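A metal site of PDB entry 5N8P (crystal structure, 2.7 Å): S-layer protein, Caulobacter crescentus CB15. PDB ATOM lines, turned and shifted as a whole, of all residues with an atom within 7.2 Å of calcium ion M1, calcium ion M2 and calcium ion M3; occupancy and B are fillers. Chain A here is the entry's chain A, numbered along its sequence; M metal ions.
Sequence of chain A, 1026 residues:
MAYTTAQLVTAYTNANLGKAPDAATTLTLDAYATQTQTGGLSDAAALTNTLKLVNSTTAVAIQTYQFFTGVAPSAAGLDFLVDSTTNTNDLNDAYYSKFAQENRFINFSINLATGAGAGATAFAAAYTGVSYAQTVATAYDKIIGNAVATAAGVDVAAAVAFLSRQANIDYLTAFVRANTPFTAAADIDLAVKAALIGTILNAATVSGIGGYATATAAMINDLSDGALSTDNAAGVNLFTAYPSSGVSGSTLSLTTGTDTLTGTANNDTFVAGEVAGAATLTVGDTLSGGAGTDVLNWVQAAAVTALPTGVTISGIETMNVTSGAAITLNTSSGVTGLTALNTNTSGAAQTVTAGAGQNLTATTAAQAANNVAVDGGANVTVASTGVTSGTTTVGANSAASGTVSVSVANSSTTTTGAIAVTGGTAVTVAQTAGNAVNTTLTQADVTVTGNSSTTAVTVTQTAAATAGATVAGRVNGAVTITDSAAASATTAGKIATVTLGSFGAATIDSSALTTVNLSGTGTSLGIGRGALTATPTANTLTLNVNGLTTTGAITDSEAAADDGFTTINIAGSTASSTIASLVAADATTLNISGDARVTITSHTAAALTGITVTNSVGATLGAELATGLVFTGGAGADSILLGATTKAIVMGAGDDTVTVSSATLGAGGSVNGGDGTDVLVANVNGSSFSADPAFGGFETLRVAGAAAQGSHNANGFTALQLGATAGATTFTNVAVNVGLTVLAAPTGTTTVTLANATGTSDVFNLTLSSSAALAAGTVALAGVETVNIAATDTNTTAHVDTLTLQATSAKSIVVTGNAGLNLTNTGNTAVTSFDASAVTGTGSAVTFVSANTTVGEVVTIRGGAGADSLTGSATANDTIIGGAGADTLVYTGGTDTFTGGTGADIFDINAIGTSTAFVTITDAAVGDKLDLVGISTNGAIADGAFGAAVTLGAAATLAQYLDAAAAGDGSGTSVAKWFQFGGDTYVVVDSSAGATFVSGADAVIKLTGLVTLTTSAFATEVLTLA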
ATOM      1  N   VAL A 613     -20.940  -9.096  33.764  1.00  0.00           N
ATOM      2  CA  VAL A 613     -21.352 -10.490  33.735  1.00  0.00           C
ATOM      3  C   VAL A 613     -20.205 -11.406  33.362  1.00  0.00           C
ATOM      4  O   VAL A 613     -19.473 -11.200  32.420  1.00  0.00           O
ATOM      5  CB  VAL A 613     -22.525 -10.728  32.790  1.00  0.00           C
ATOM      6  CG1 VAL A 613     -23.141 -12.072  33.095  1.00  0.00           C
ATOM      7  CG2 VAL A 613     -23.535  -9.616  32.974  1.00  0.00           C
ATOM      8  N   ASN A 615     -21.017 -14.775  34.163  1.00  0.00           N
ATOM      9  CA  ASN A 615     -21.848 -15.972  34.258  1.00  0.00           C
ATOM     10  C   ASN A 615     -21.954 -16.767  32.958  1.00  0.00           C
ATOM     11  O   ASN A 615     -22.174 -16.195  31.924  1.00  0.00           O
ATOM     12  CB  ASN A 615     -23.245 -15.543  34.738  1.00  0.00           C
ATOM     13  CG  ASN A 615     -24.175 -16.728  34.983  1.00  0.00           C
ATOM     14  OD1 ASN A 615     -24.506 -17.469  34.066  1.00  0.00           O
ATOM     15  ND2 ASN A 615     -24.622 -16.877  36.225  1.00  0.00           N
ATOM     16  N   VAL A 617     -24.263 -19.127  31.783  1.00  0.00           N
ATOM     17  CA  VAL A 617     -25.548 -19.171  31.090  1.00  0.00           C
ATOM     18  C   VAL A 617     -25.890 -17.767  30.631  1.00  0.00           C
ATOM     19  O   VAL A 617     -26.422 -17.576  29.559  1.00  0.00           O
ATOM     20  CB  VAL A 617     -26.630 -19.852  31.957  1.00  0.00           C
ATOM     21  CG1 VAL A 617     -28.047 -19.674  31.394  1.00  0.00           C
ATOM     22  CG2 VAL A 617     -26.289 -21.329  32.119  1.00  0.00           C
ATOM     23  N   GLY A 618     -25.538 -16.789  31.454  1.00  0.00           N
ATOM     24  CA  GLY A 618     -25.790 -15.394  31.132  1.00  0.00           C
ATOM     25  C   GLY A 618     -26.610 -14.675  32.162  1.00  0.00           C
ATOM     26  O   GLY A 618     -27.007 -15.249  33.175  1.00  0.00           O
ATOM     27  N   PHE A 631     -21.354  -1.659  30.422  1.00  0.00           N
ATOM     28  CA  PHE A 631     -21.764  -3.033  30.612  1.00  0.00           C
ATOM     29  C   PHE A 631     -20.807  -3.967  29.904  1.00  0.00           C
ATOM     30  O   PHE A 631     -20.462  -3.736  28.791  1.00  0.00           O
ATOM     31  CB  PHE A 631     -23.194  -3.248  30.075  1.00  0.00           C
ATOM     32  CG  PHE A 631     -23.658  -4.689  30.151  1.00  0.00           C
ATOM     33  CD1 PHE A 631     -24.421  -5.129  31.222  1.00  0.00           C
ATOM     34  CD2 PHE A 631     -23.302  -5.615  29.162  1.00  0.00           C
ATOM     35  CE1 PHE A 631     -24.828  -6.440  31.324  1.00  0.00           C
ATOM     36  CE2 PHE A 631     -23.705  -6.940  29.247  1.00  0.00           C
ATOM     37  CZ  PHE A 631     -24.470  -7.346  30.325  1.00  0.00           C
ATOM     38  N   THR A 632     -20.439  -5.050  30.548  1.00  0.00           N
ATOM     39  CA  THR A 632     -19.574  -6.054  29.912  1.00  0.00           C
ATOM     40  C   THR A 632     -20.171  -7.460  30.080  1.00  0.00           C
ATOM     41  O   THR A 632     -20.347  -7.910  31.187  1.00  0.00           O
ATOM     42  CB  THR A 632     -18.149  -5.940  30.497  1.00  0.00           C
ATOM     43  OG1 THR A 632     -17.807  -4.562  30.600  1.00  0.00           O
ATOM     44  CG2 THR A 632     -17.135  -6.689  29.652  1.00  0.00           C
ATOM     45  N   GLY A 633     -20.520  -8.117  28.982  1.00  0.00           N
ATOM     46  CA  GLY A 633     -20.984  -9.518  29.017  1.00  0.00           C
ATOM     47  C   GLY A 633     -19.822 -10.506  29.107  1.00  0.00           C
ATOM     48  O   GLY A 633     -18.642 -10.103  29.048  1.00  0.00           O
ATOM     49  N   GLY A 634     -20.141 -11.792  29.251  1.00  0.00           N
ATOM     50  CA  GLY A 634     -19.149 -12.896  29.228  1.00  0.00           C
ATOM     51  C   GLY A 634     -19.603 -13.886  28.202  1.00  0.00           C
ATOM     52  O   GLY A 634     -20.322 -13.485  27.270  1.00  0.00           O
ATOM     53  N   ALA A 635     -19.221 -15.169  28.307  1.00  0.00           N
ATOM     54  CA  ALA A 635     -19.854 -16.237  27.506  1.00  0.00           C
ATOM     55  C   ALA A 635     -21.348 -16.258  27.847  1.00  0.00           C
ATOM     56  O   ALA A 635     -21.769 -15.601  28.775  1.00  0.00           O
ATOM     57  CB  ALA A 635     -19.189 -17.597  27.746  1.00  0.00           C
ATOM     58  N   GLY A 636     -22.152 -16.961  27.065  1.00  0.00           N
ATOM     59  CA  GLY A 636     -23.573 -17.092  27.412  1.00  0.00           C
ATOM     60  C   GLY A 636     -24.483 -15.893  27.206  1.00  0.00           C
ATOM     61  O   GLY A 636     -24.061 -14.726  27.269  1.00  0.00           O
ATOM     62  N   ALA A 637     -25.758 -16.202  26.987  1.00  0.00           N
ATOM     63  CA  ALA A 637     -26.754 -15.270  26.474  1.00  0.00           C
ATOM     64  C   ALA A 637     -26.995 -14.142  27.449  1.00  0.00           C
ATOM     65  O   ALA A 637     -27.860 -14.257  28.297  1.00  0.00           O
ATOM     66  CB  ALA A 637     -28.069 -15.995  26.117  1.00  0.00           C
ATOM     67  N   ASP A 638     -26.213 -13.078  27.373  1.00  0.00           N
ATOM     68  CA  ASP A 638     -26.498 -11.928  28.215  1.00  0.00           C
ATOM     69  C   ASP A 638     -27.552 -11.066  27.500  1.00  0.00           C
ATOM     70  O   ASP A 638     -27.713 -11.202  26.286  1.00  0.00           O
ATOM     71  CB  ASP A 638     -25.210 -11.170  28.598  1.00  0.00           C
ATOM     72  CG  ASP A 638     -24.039 -12.106  29.004  1.00  0.00           C
ATOM     73  OD1 ASP A 638     -24.108 -12.798  30.031  1.00  0.00           O
ATOM     74  OD2 ASP A 638     -23.030 -12.157  28.270  1.00  0.00           O
ATOM     75  N   SER A 639     -28.306 -10.223  28.224  1.00  0.00           N
ATOM     76  CA  SER A 639     -29.441  -9.489  27.604  1.00  0.00           C
ATOM     77  C   SER A 639     -29.935  -8.219  28.303  1.00  0.00           C
ATOM     78  O   SER A 639     -30.505  -8.282  29.393  1.00  0.00           O
ATOM     79  CB  SER A 639     -30.610 -10.414  27.331  1.00  0.00           C
ATOM     80  OG  SER A 639     -31.792  -9.664  27.187  1.00  0.00           O
ATOM     81  N   VAL A 650     -19.814  -3.915  25.564  1.00  0.00           N
ATOM     82  CA  VAL A 650     -19.343  -5.166  24.976  1.00  0.00           C
ATOM     83  C   VAL A 650     -20.217  -6.283  25.481  1.00  0.00           C
ATOM     84  O   VAL A 650     -20.675  -6.225  26.596  1.00  0.00           O
ATOM     85  CB  VAL A 650     -17.847  -5.498  25.256  1.00  0.00           C
ATOM     86  CG1 VAL A 650     -17.370  -6.646  24.334  1.00  0.00           C
ATOM     87  CG2 VAL A 650     -16.974  -4.254  25.047  1.00  0.00           C
ATOM     88  N   MET A 651     -20.442  -7.304  24.652  1.00  0.00           N
ATOM     89  CA  MET A 651     -21.396  -8.322  24.941  1.00  0.00           C
ATOM     90  C   MET A 651     -20.776  -9.678  25.123  1.00  0.00           C
ATOM     91  O   MET A 651     -21.465 -10.596  25.595  1.00  0.00           O
ATOM     92  CB  MET A 651     -22.418  -8.378  23.843  1.00  0.00           C
ATOM     93  CG  MET A 651     -23.830  -8.253  24.320  1.00  0.00           C
ATOM     94  SD  MET A 651     -24.079  -6.746  25.248  1.00  0.00           S
ATOM     95  CE  MET A 651     -25.676  -7.138  25.996  1.00  0.00           C
ATOM     96  N   GLY A 652     -19.493  -9.821  24.762  1.00  0.00           N
ATOM     97  CA  GLY A 652     -18.753 -11.099  24.930  1.00  0.00           C
ATOM     98  C   GLY A 652     -19.232 -12.203  23.997  1.00  0.00           C
ATOM     99  O   GLY A 652     -19.950 -11.931  23.034  1.00  0.00           O
ATOM    100  N   ALA A 653     -18.848 -13.446  24.289  1.00  0.00           N
ATOM    101  CA  ALA A 653     -19.277 -14.621  23.501  1.00  0.00           C
ATOM    102  C   ALA A 653     -20.749 -15.000  23.749  1.00  0.00           C
ATOM    103  O   ALA A 653     -21.446 -14.310  24.482  1.00  0.00           O
ATOM    104  CB  ALA A 653     -18.348 -15.826  23.738  1.00  0.00           C
ATOM    105  N   GLY A 654     -21.220 -16.074  23.098  1.00  0.00           N
ATOM    106  CA  GLY A 654     -22.583 -16.579  23.258  1.00  0.00           C
ATOM    107  C   GLY A 654     -23.696 -15.736  22.662  1.00  0.00           C
ATOM    108  O   GLY A 654     -23.483 -14.597  22.252  1.00  0.00           O
ATOM    109  N   ASP A 655     -24.904 -16.258  22.636  1.00  0.00           N
ATOM    110  CA  ASP A 655     -25.965 -15.631  21.884  1.00  0.00           C
ATOM    111  C   ASP A 655     -26.721 -14.511  22.617  1.00  0.00           C
ATOM    112  O   ASP A 655     -27.764 -14.719  23.252  1.00  0.00           O
ATOM    113  CB  ASP A 655     -26.851 -16.724  21.296  1.00  0.00           C
ATOM    114  CG  ASP A 655     -26.077 -17.628  20.332  1.00  0.00           C
ATOM    115  OD1 ASP A 655     -26.764 -18.463  19.691  1.00  0.00           O
ATOM    116  OD2 ASP A 655     -24.813 -17.520  20.191  1.00  0.00           O
ATOM    117  N   ASP A 656     -26.170 -13.308  22.488  1.00  0.00           N
ATOM    118  CA  ASP A 656     -26.583 -12.153  23.296  1.00  0.00           C
ATOM    119  C   ASP A 656     -27.737 -11.375  22.685  1.00  0.00           C
ATOM    120  O   ASP A 656     -28.079 -11.610  21.537  1.00  0.00           O
ATOM    121  CB  ASP A 656     -25.378 -11.245  23.475  1.00  0.00           C
ATOM    122  CG  ASP A 656     -24.269 -11.890  24.289  1.00  0.00           C
ATOM    123  OD1 ASP A 656     -24.461 -12.123  25.506  1.00  0.00           O
ATOM    124  OD2 ASP A 656     -23.167 -12.149  23.739  1.00  0.00           O
ATOM    125  N   THR A 657     -28.328 -10.444  23.433  1.00  0.00           N
ATOM    126  CA  THR A 657     -29.506  -9.666  22.943  1.00  0.00           C
ATOM    127  C   THR A 657     -29.548  -8.224  23.496  1.00  0.00           C
ATOM    128  O   THR A 657     -29.907  -8.029  24.667  1.00  0.00           O
ATOM    129  CB  THR A 657     -30.839 -10.349  23.337  1.00  0.00           C
ATOM    130  OG1 THR A 657     -30.776 -11.720  22.996  1.00  0.00           O
ATOM    131  CG2 THR A 657     -32.016  -9.735  22.535  1.00  0.00           C
ATOM    132  N   ASN A 672     -20.869  -3.579  20.811  1.00  0.00           N
ATOM    133  CA  ASN A 672     -20.412  -4.702  20.031  1.00  0.00           C
ATOM    134  C   ASN A 672     -21.006  -6.012  20.577  1.00  0.00           C
ATOM    135  O   ASN A 672     -20.795  -6.356  21.724  1.00  0.00           O
ATOM    136  CB  ASN A 672     -18.858  -4.718  19.942  1.00  0.00           C
ATOM    137  CG  ASN A 672     -18.292  -6.044  19.372  1.00  0.00           C
ATOM    138  OD1 ASN A 672     -18.771  -6.587  18.385  1.00  0.00           O
ATOM    139  ND2 ASN A 672     -17.231  -6.539  19.995  1.00  0.00           N
ATOM    140  N   GLY A 673     -21.774  -6.714  19.750  1.00  0.00           N
ATOM    141  CA  GLY A 673     -22.282  -8.037  20.047  1.00  0.00           C
ATOM    142  C   GLY A 673     -21.278  -9.143  20.342  1.00  0.00           C
ATOM    143  O   GLY A 673     -21.689 -10.183  20.856  1.00  0.00           O
ATOM    144  N   GLY A 674     -19.970  -8.949  20.045  1.00  0.00           N
ATOM    145  CA  GLY A 674     -18.923  -9.986  20.238  1.00  0.00           C
ATOM    146  C   GLY A 674     -19.167 -11.281  19.427  1.00  0.00           C
ATOM    147  O   GLY A 674     -19.952 -11.299  18.493  1.00  0.00           O
ATOM    148  N   ASP A 675     -18.488 -12.358  19.782  1.00  0.00           N
ATOM    149  CA  ASP A 675     -18.677 -13.659  19.118  1.00  0.00           C
ATOM    150  C   ASP A 675     -20.081 -14.265  19.292  1.00  0.00           C
ATOM    151  O   ASP A 675     -20.799 -13.927  20.251  1.00  0.00           O
ATOM    152  CB  ASP A 675     -17.662 -14.693  19.616  1.00  0.00           C
ATOM    153  CG  ASP A 675     -16.233 -14.327  19.328  1.00  0.00           C
ATOM    154  OD1 ASP A 675     -15.994 -13.164  18.877  1.00  0.00           O
ATOM    155  OD2 ASP A 675     -15.373 -15.211  19.574  1.00  0.00           O
ATOM    156  N   GLY A 676     -20.443 -15.166  18.368  1.00  0.00           N
ATOM    157  CA  GLY A 676     -21.731 -15.889  18.413  1.00  0.00           C
ATOM    158  C   GLY A 676     -22.856 -15.177  17.687  1.00  0.00           C
ATOM    159  O   GLY A 676     -22.668 -14.076  17.153  1.00  0.00           O
ATOM    160  N   THR A 677     -24.029 -15.791  17.658  1.00  0.00           N
ATOM    161  CA  THR A 677     -25.144 -15.213  16.923  1.00  0.00           C
ATOM    162  C   THR A 677     -25.897 -14.313  17.860  1.00  0.00           C
ATOM    163  O   THR A 677     -26.564 -14.789  18.782  1.00  0.00           O
ATOM    164  CB  THR A 677     -26.058 -16.314  16.358  1.00  0.00           C
ATOM    165  OG1 THR A 677     -25.229 -17.300  15.736  1.00  0.00           O
ATOM    166  CG2 THR A 677     -27.009 -15.754  15.320  1.00  0.00           C
ATOM    167  N   ASP A 678     -25.813 -13.005  17.627  1.00  0.00           N
ATOM    168  CA  ASP A 678     -26.378 -12.033  18.566  1.00  0.00           C
ATOM    169  C   ASP A 678     -27.504 -11.268  17.940  1.00  0.00           C
ATOM    170  O   ASP A 678     -27.396 -10.851  16.801  1.00  0.00           O
ATOM    171  CB  ASP A 678     -25.296 -11.060  19.036  1.00  0.00           C
ATOM    172  CG  ASP A 678     -24.018 -11.755  19.459  1.00  0.00           C
ATOM    173  OD1 ASP A 678     -23.988 -12.309  20.586  1.00  0.00           O
ATOM    174  OD2 ASP A 678     -23.028 -11.722  18.669  1.00  0.00           O
ATOM    175  N   GLY A 696     -21.667  -3.285  15.932  1.00  0.00           N
ATOM    176  CA  GLY A 696     -20.897  -4.327  15.228  1.00  0.00           C
ATOM    177  C   GLY A 696     -21.101  -5.694  15.878  1.00  0.00           C
ATOM    178  O   GLY A 696     -21.527  -5.754  17.049  1.00  0.00           O
ATOM    179  N   GLY A 697     -20.816  -6.790  15.160  1.00  0.00           N
ATOM    180  CA  GLY A 697     -20.916  -8.145  15.762  1.00  0.00           C
ATOM    181  C   GLY A 697     -22.308  -8.732  15.935  1.00  0.00           C
ATOM    182  O   GLY A 697     -22.492  -9.789  16.560  1.00  0.00           O
ATOM    183  N   PHE A 698     -23.309  -8.049  15.367  1.00  0.00           N
ATOM    184  CA  PHE A 698     -24.695  -8.533  15.331  1.00  0.00           C
ATOM    185  C   PHE A 698     -25.017  -9.333  14.063  1.00  0.00           C
ATOM    186  O   PHE A 698     -24.423  -9.102  13.025  1.00  0.00           O
ATOM    187  CB  PHE A 698     -25.665  -7.356  15.530  1.00  0.00           C
ATOM    188  CG  PHE A 698     -25.644  -6.825  16.922  1.00  0.00           C
ATOM    189  CD1 PHE A 698     -26.394  -7.451  17.927  1.00  0.00           C
ATOM    190  CD2 PHE A 698     -24.824  -5.760  17.257  1.00  0.00           C
ATOM    191  CE1 PHE A 698     -26.337  -6.994  19.240  1.00  0.00           C
ATOM    192  CE2 PHE A 698     -24.774  -5.295  18.556  1.00  0.00           C
ATOM    193  CZ  PHE A 698     -25.527  -5.925  19.553  1.00  0.00           C
ATOM    194  N   GLU A 699     -25.938 -10.280  14.183  1.00  0.00           N
ATOM    195  CA  GLU A 699     -26.227 -11.214  13.092  1.00  0.00           C
ATOM    196  C   GLU A 699     -27.696 -11.231  12.761  1.00  0.00           C
ATOM    197  O   GLU A 699     -28.044 -11.588  11.648  1.00  0.00           O
ATOM    198  CB  GLU A 699     -25.768 -12.618  13.459  1.00  0.00           C
ATOM    199  CG  GLU A 699     -24.271 -12.836  13.377  1.00  0.00           C
ATOM    200  CD  GLU A 699     -23.490 -12.283  14.567  1.00  0.00           C
ATOM    201  OE1 GLU A 699     -24.043 -11.965  15.657  1.00  0.00           O
ATOM    202  OE2 GLU A 699     -22.245 -12.169  14.417  1.00  0.00           O
HETATM  203 CA    CA M   1     -22.052 -12.492  21.750  1.00  0.00          CA
HETATM  204 CA    CA M   2     -22.264 -12.864  26.337  1.00  0.00          CA
HETATM  205 CA    CA M   3     -21.492 -11.981  16.596  1.00  0.00          CA
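Eight residues have an atom within 4 Å of calcium ion M1: Gly 652, Ala 653, Gly 654, Asp 656, Gly 673, Gly 674, Asp 675 and Asp 678.
Calcium ion M2 is bound by the side-chain carboxylate (OD2) of Asp 638, 2.2 Å away. Calcium ion M2 is bound by O of Gly 634 (2.2 Å). The side-chain carboxylate (OD1) of Asp 656 binds calcium ion M2. Calcium ion M2 is bound by O of Ala 653 (2.5 Å). Calcium ion M2 is bound by the backbone carbonyl oxygen (O) of Met 651. O of Gly 636 binds calcium ion M2, at 2.8 Å. OD2 of Asp 656 is bound to calcium ion M2, 2.8 Å away.
The backbone carbonyl oxygen (O) of Val 613 is in hydrogen-bond range of the backbone NH (N) of Gly 634 (3.3 Å). The backbone NH of Thr 657 is in hydrogen-bond range of the backbone carbonyl oxygen of Asp 638 (3.0 Å). The backbone NH (N) of Met 651 sits at hydrogen-bond distance from the backbone carbonyl oxygen (O) of Asn 672. The side-chain amide oxygen (OD1) of Asn 672 sits at hydrogen-bond distance from the backbone NH (N) of Gly 674 (3.1 Å). The backbone NH (N) of Gly 673 lies within hydrogen-bond range of the backbone carbonyl oxygen (O) of Gly 696 (2.9 Å).
Calcium ion M3 is bound by OE2 of Glu 699 (2.3 Å), O of Gly 697 (2.4 Å), O of Gly 676 (2.5 Å), O of Gly 674 (2.5 Å), OD2 of Asp 678 (2.6 Å) and OE1 of Glu 699 (2.7 Å).
Ala 635 touches calcium ion M2 (O to CA, 3.7 Å). Eight residues have an atom within 4 Å of calcium ion M2: Gly 634, Ala 635, Gly 636, Asp 638, Met 651, Gly 652, Ala 653 and Asp 656. Along chain A the residues within 4 Å of calcium ion M2 span positions 634 to 656.
Calcium ion M1 is bound by OD1 of Asp 678 (2.3 Å), OD2 of Asp 656 (2.3 Å), O of Asp 675 (2.4 Å), O of Gly 673 (2.5 Å), O of Gly 652 (2.5 Å) and O of Gly 654 (2.6 Å). Calcium ion M1 has six donor atoms within binding distance.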
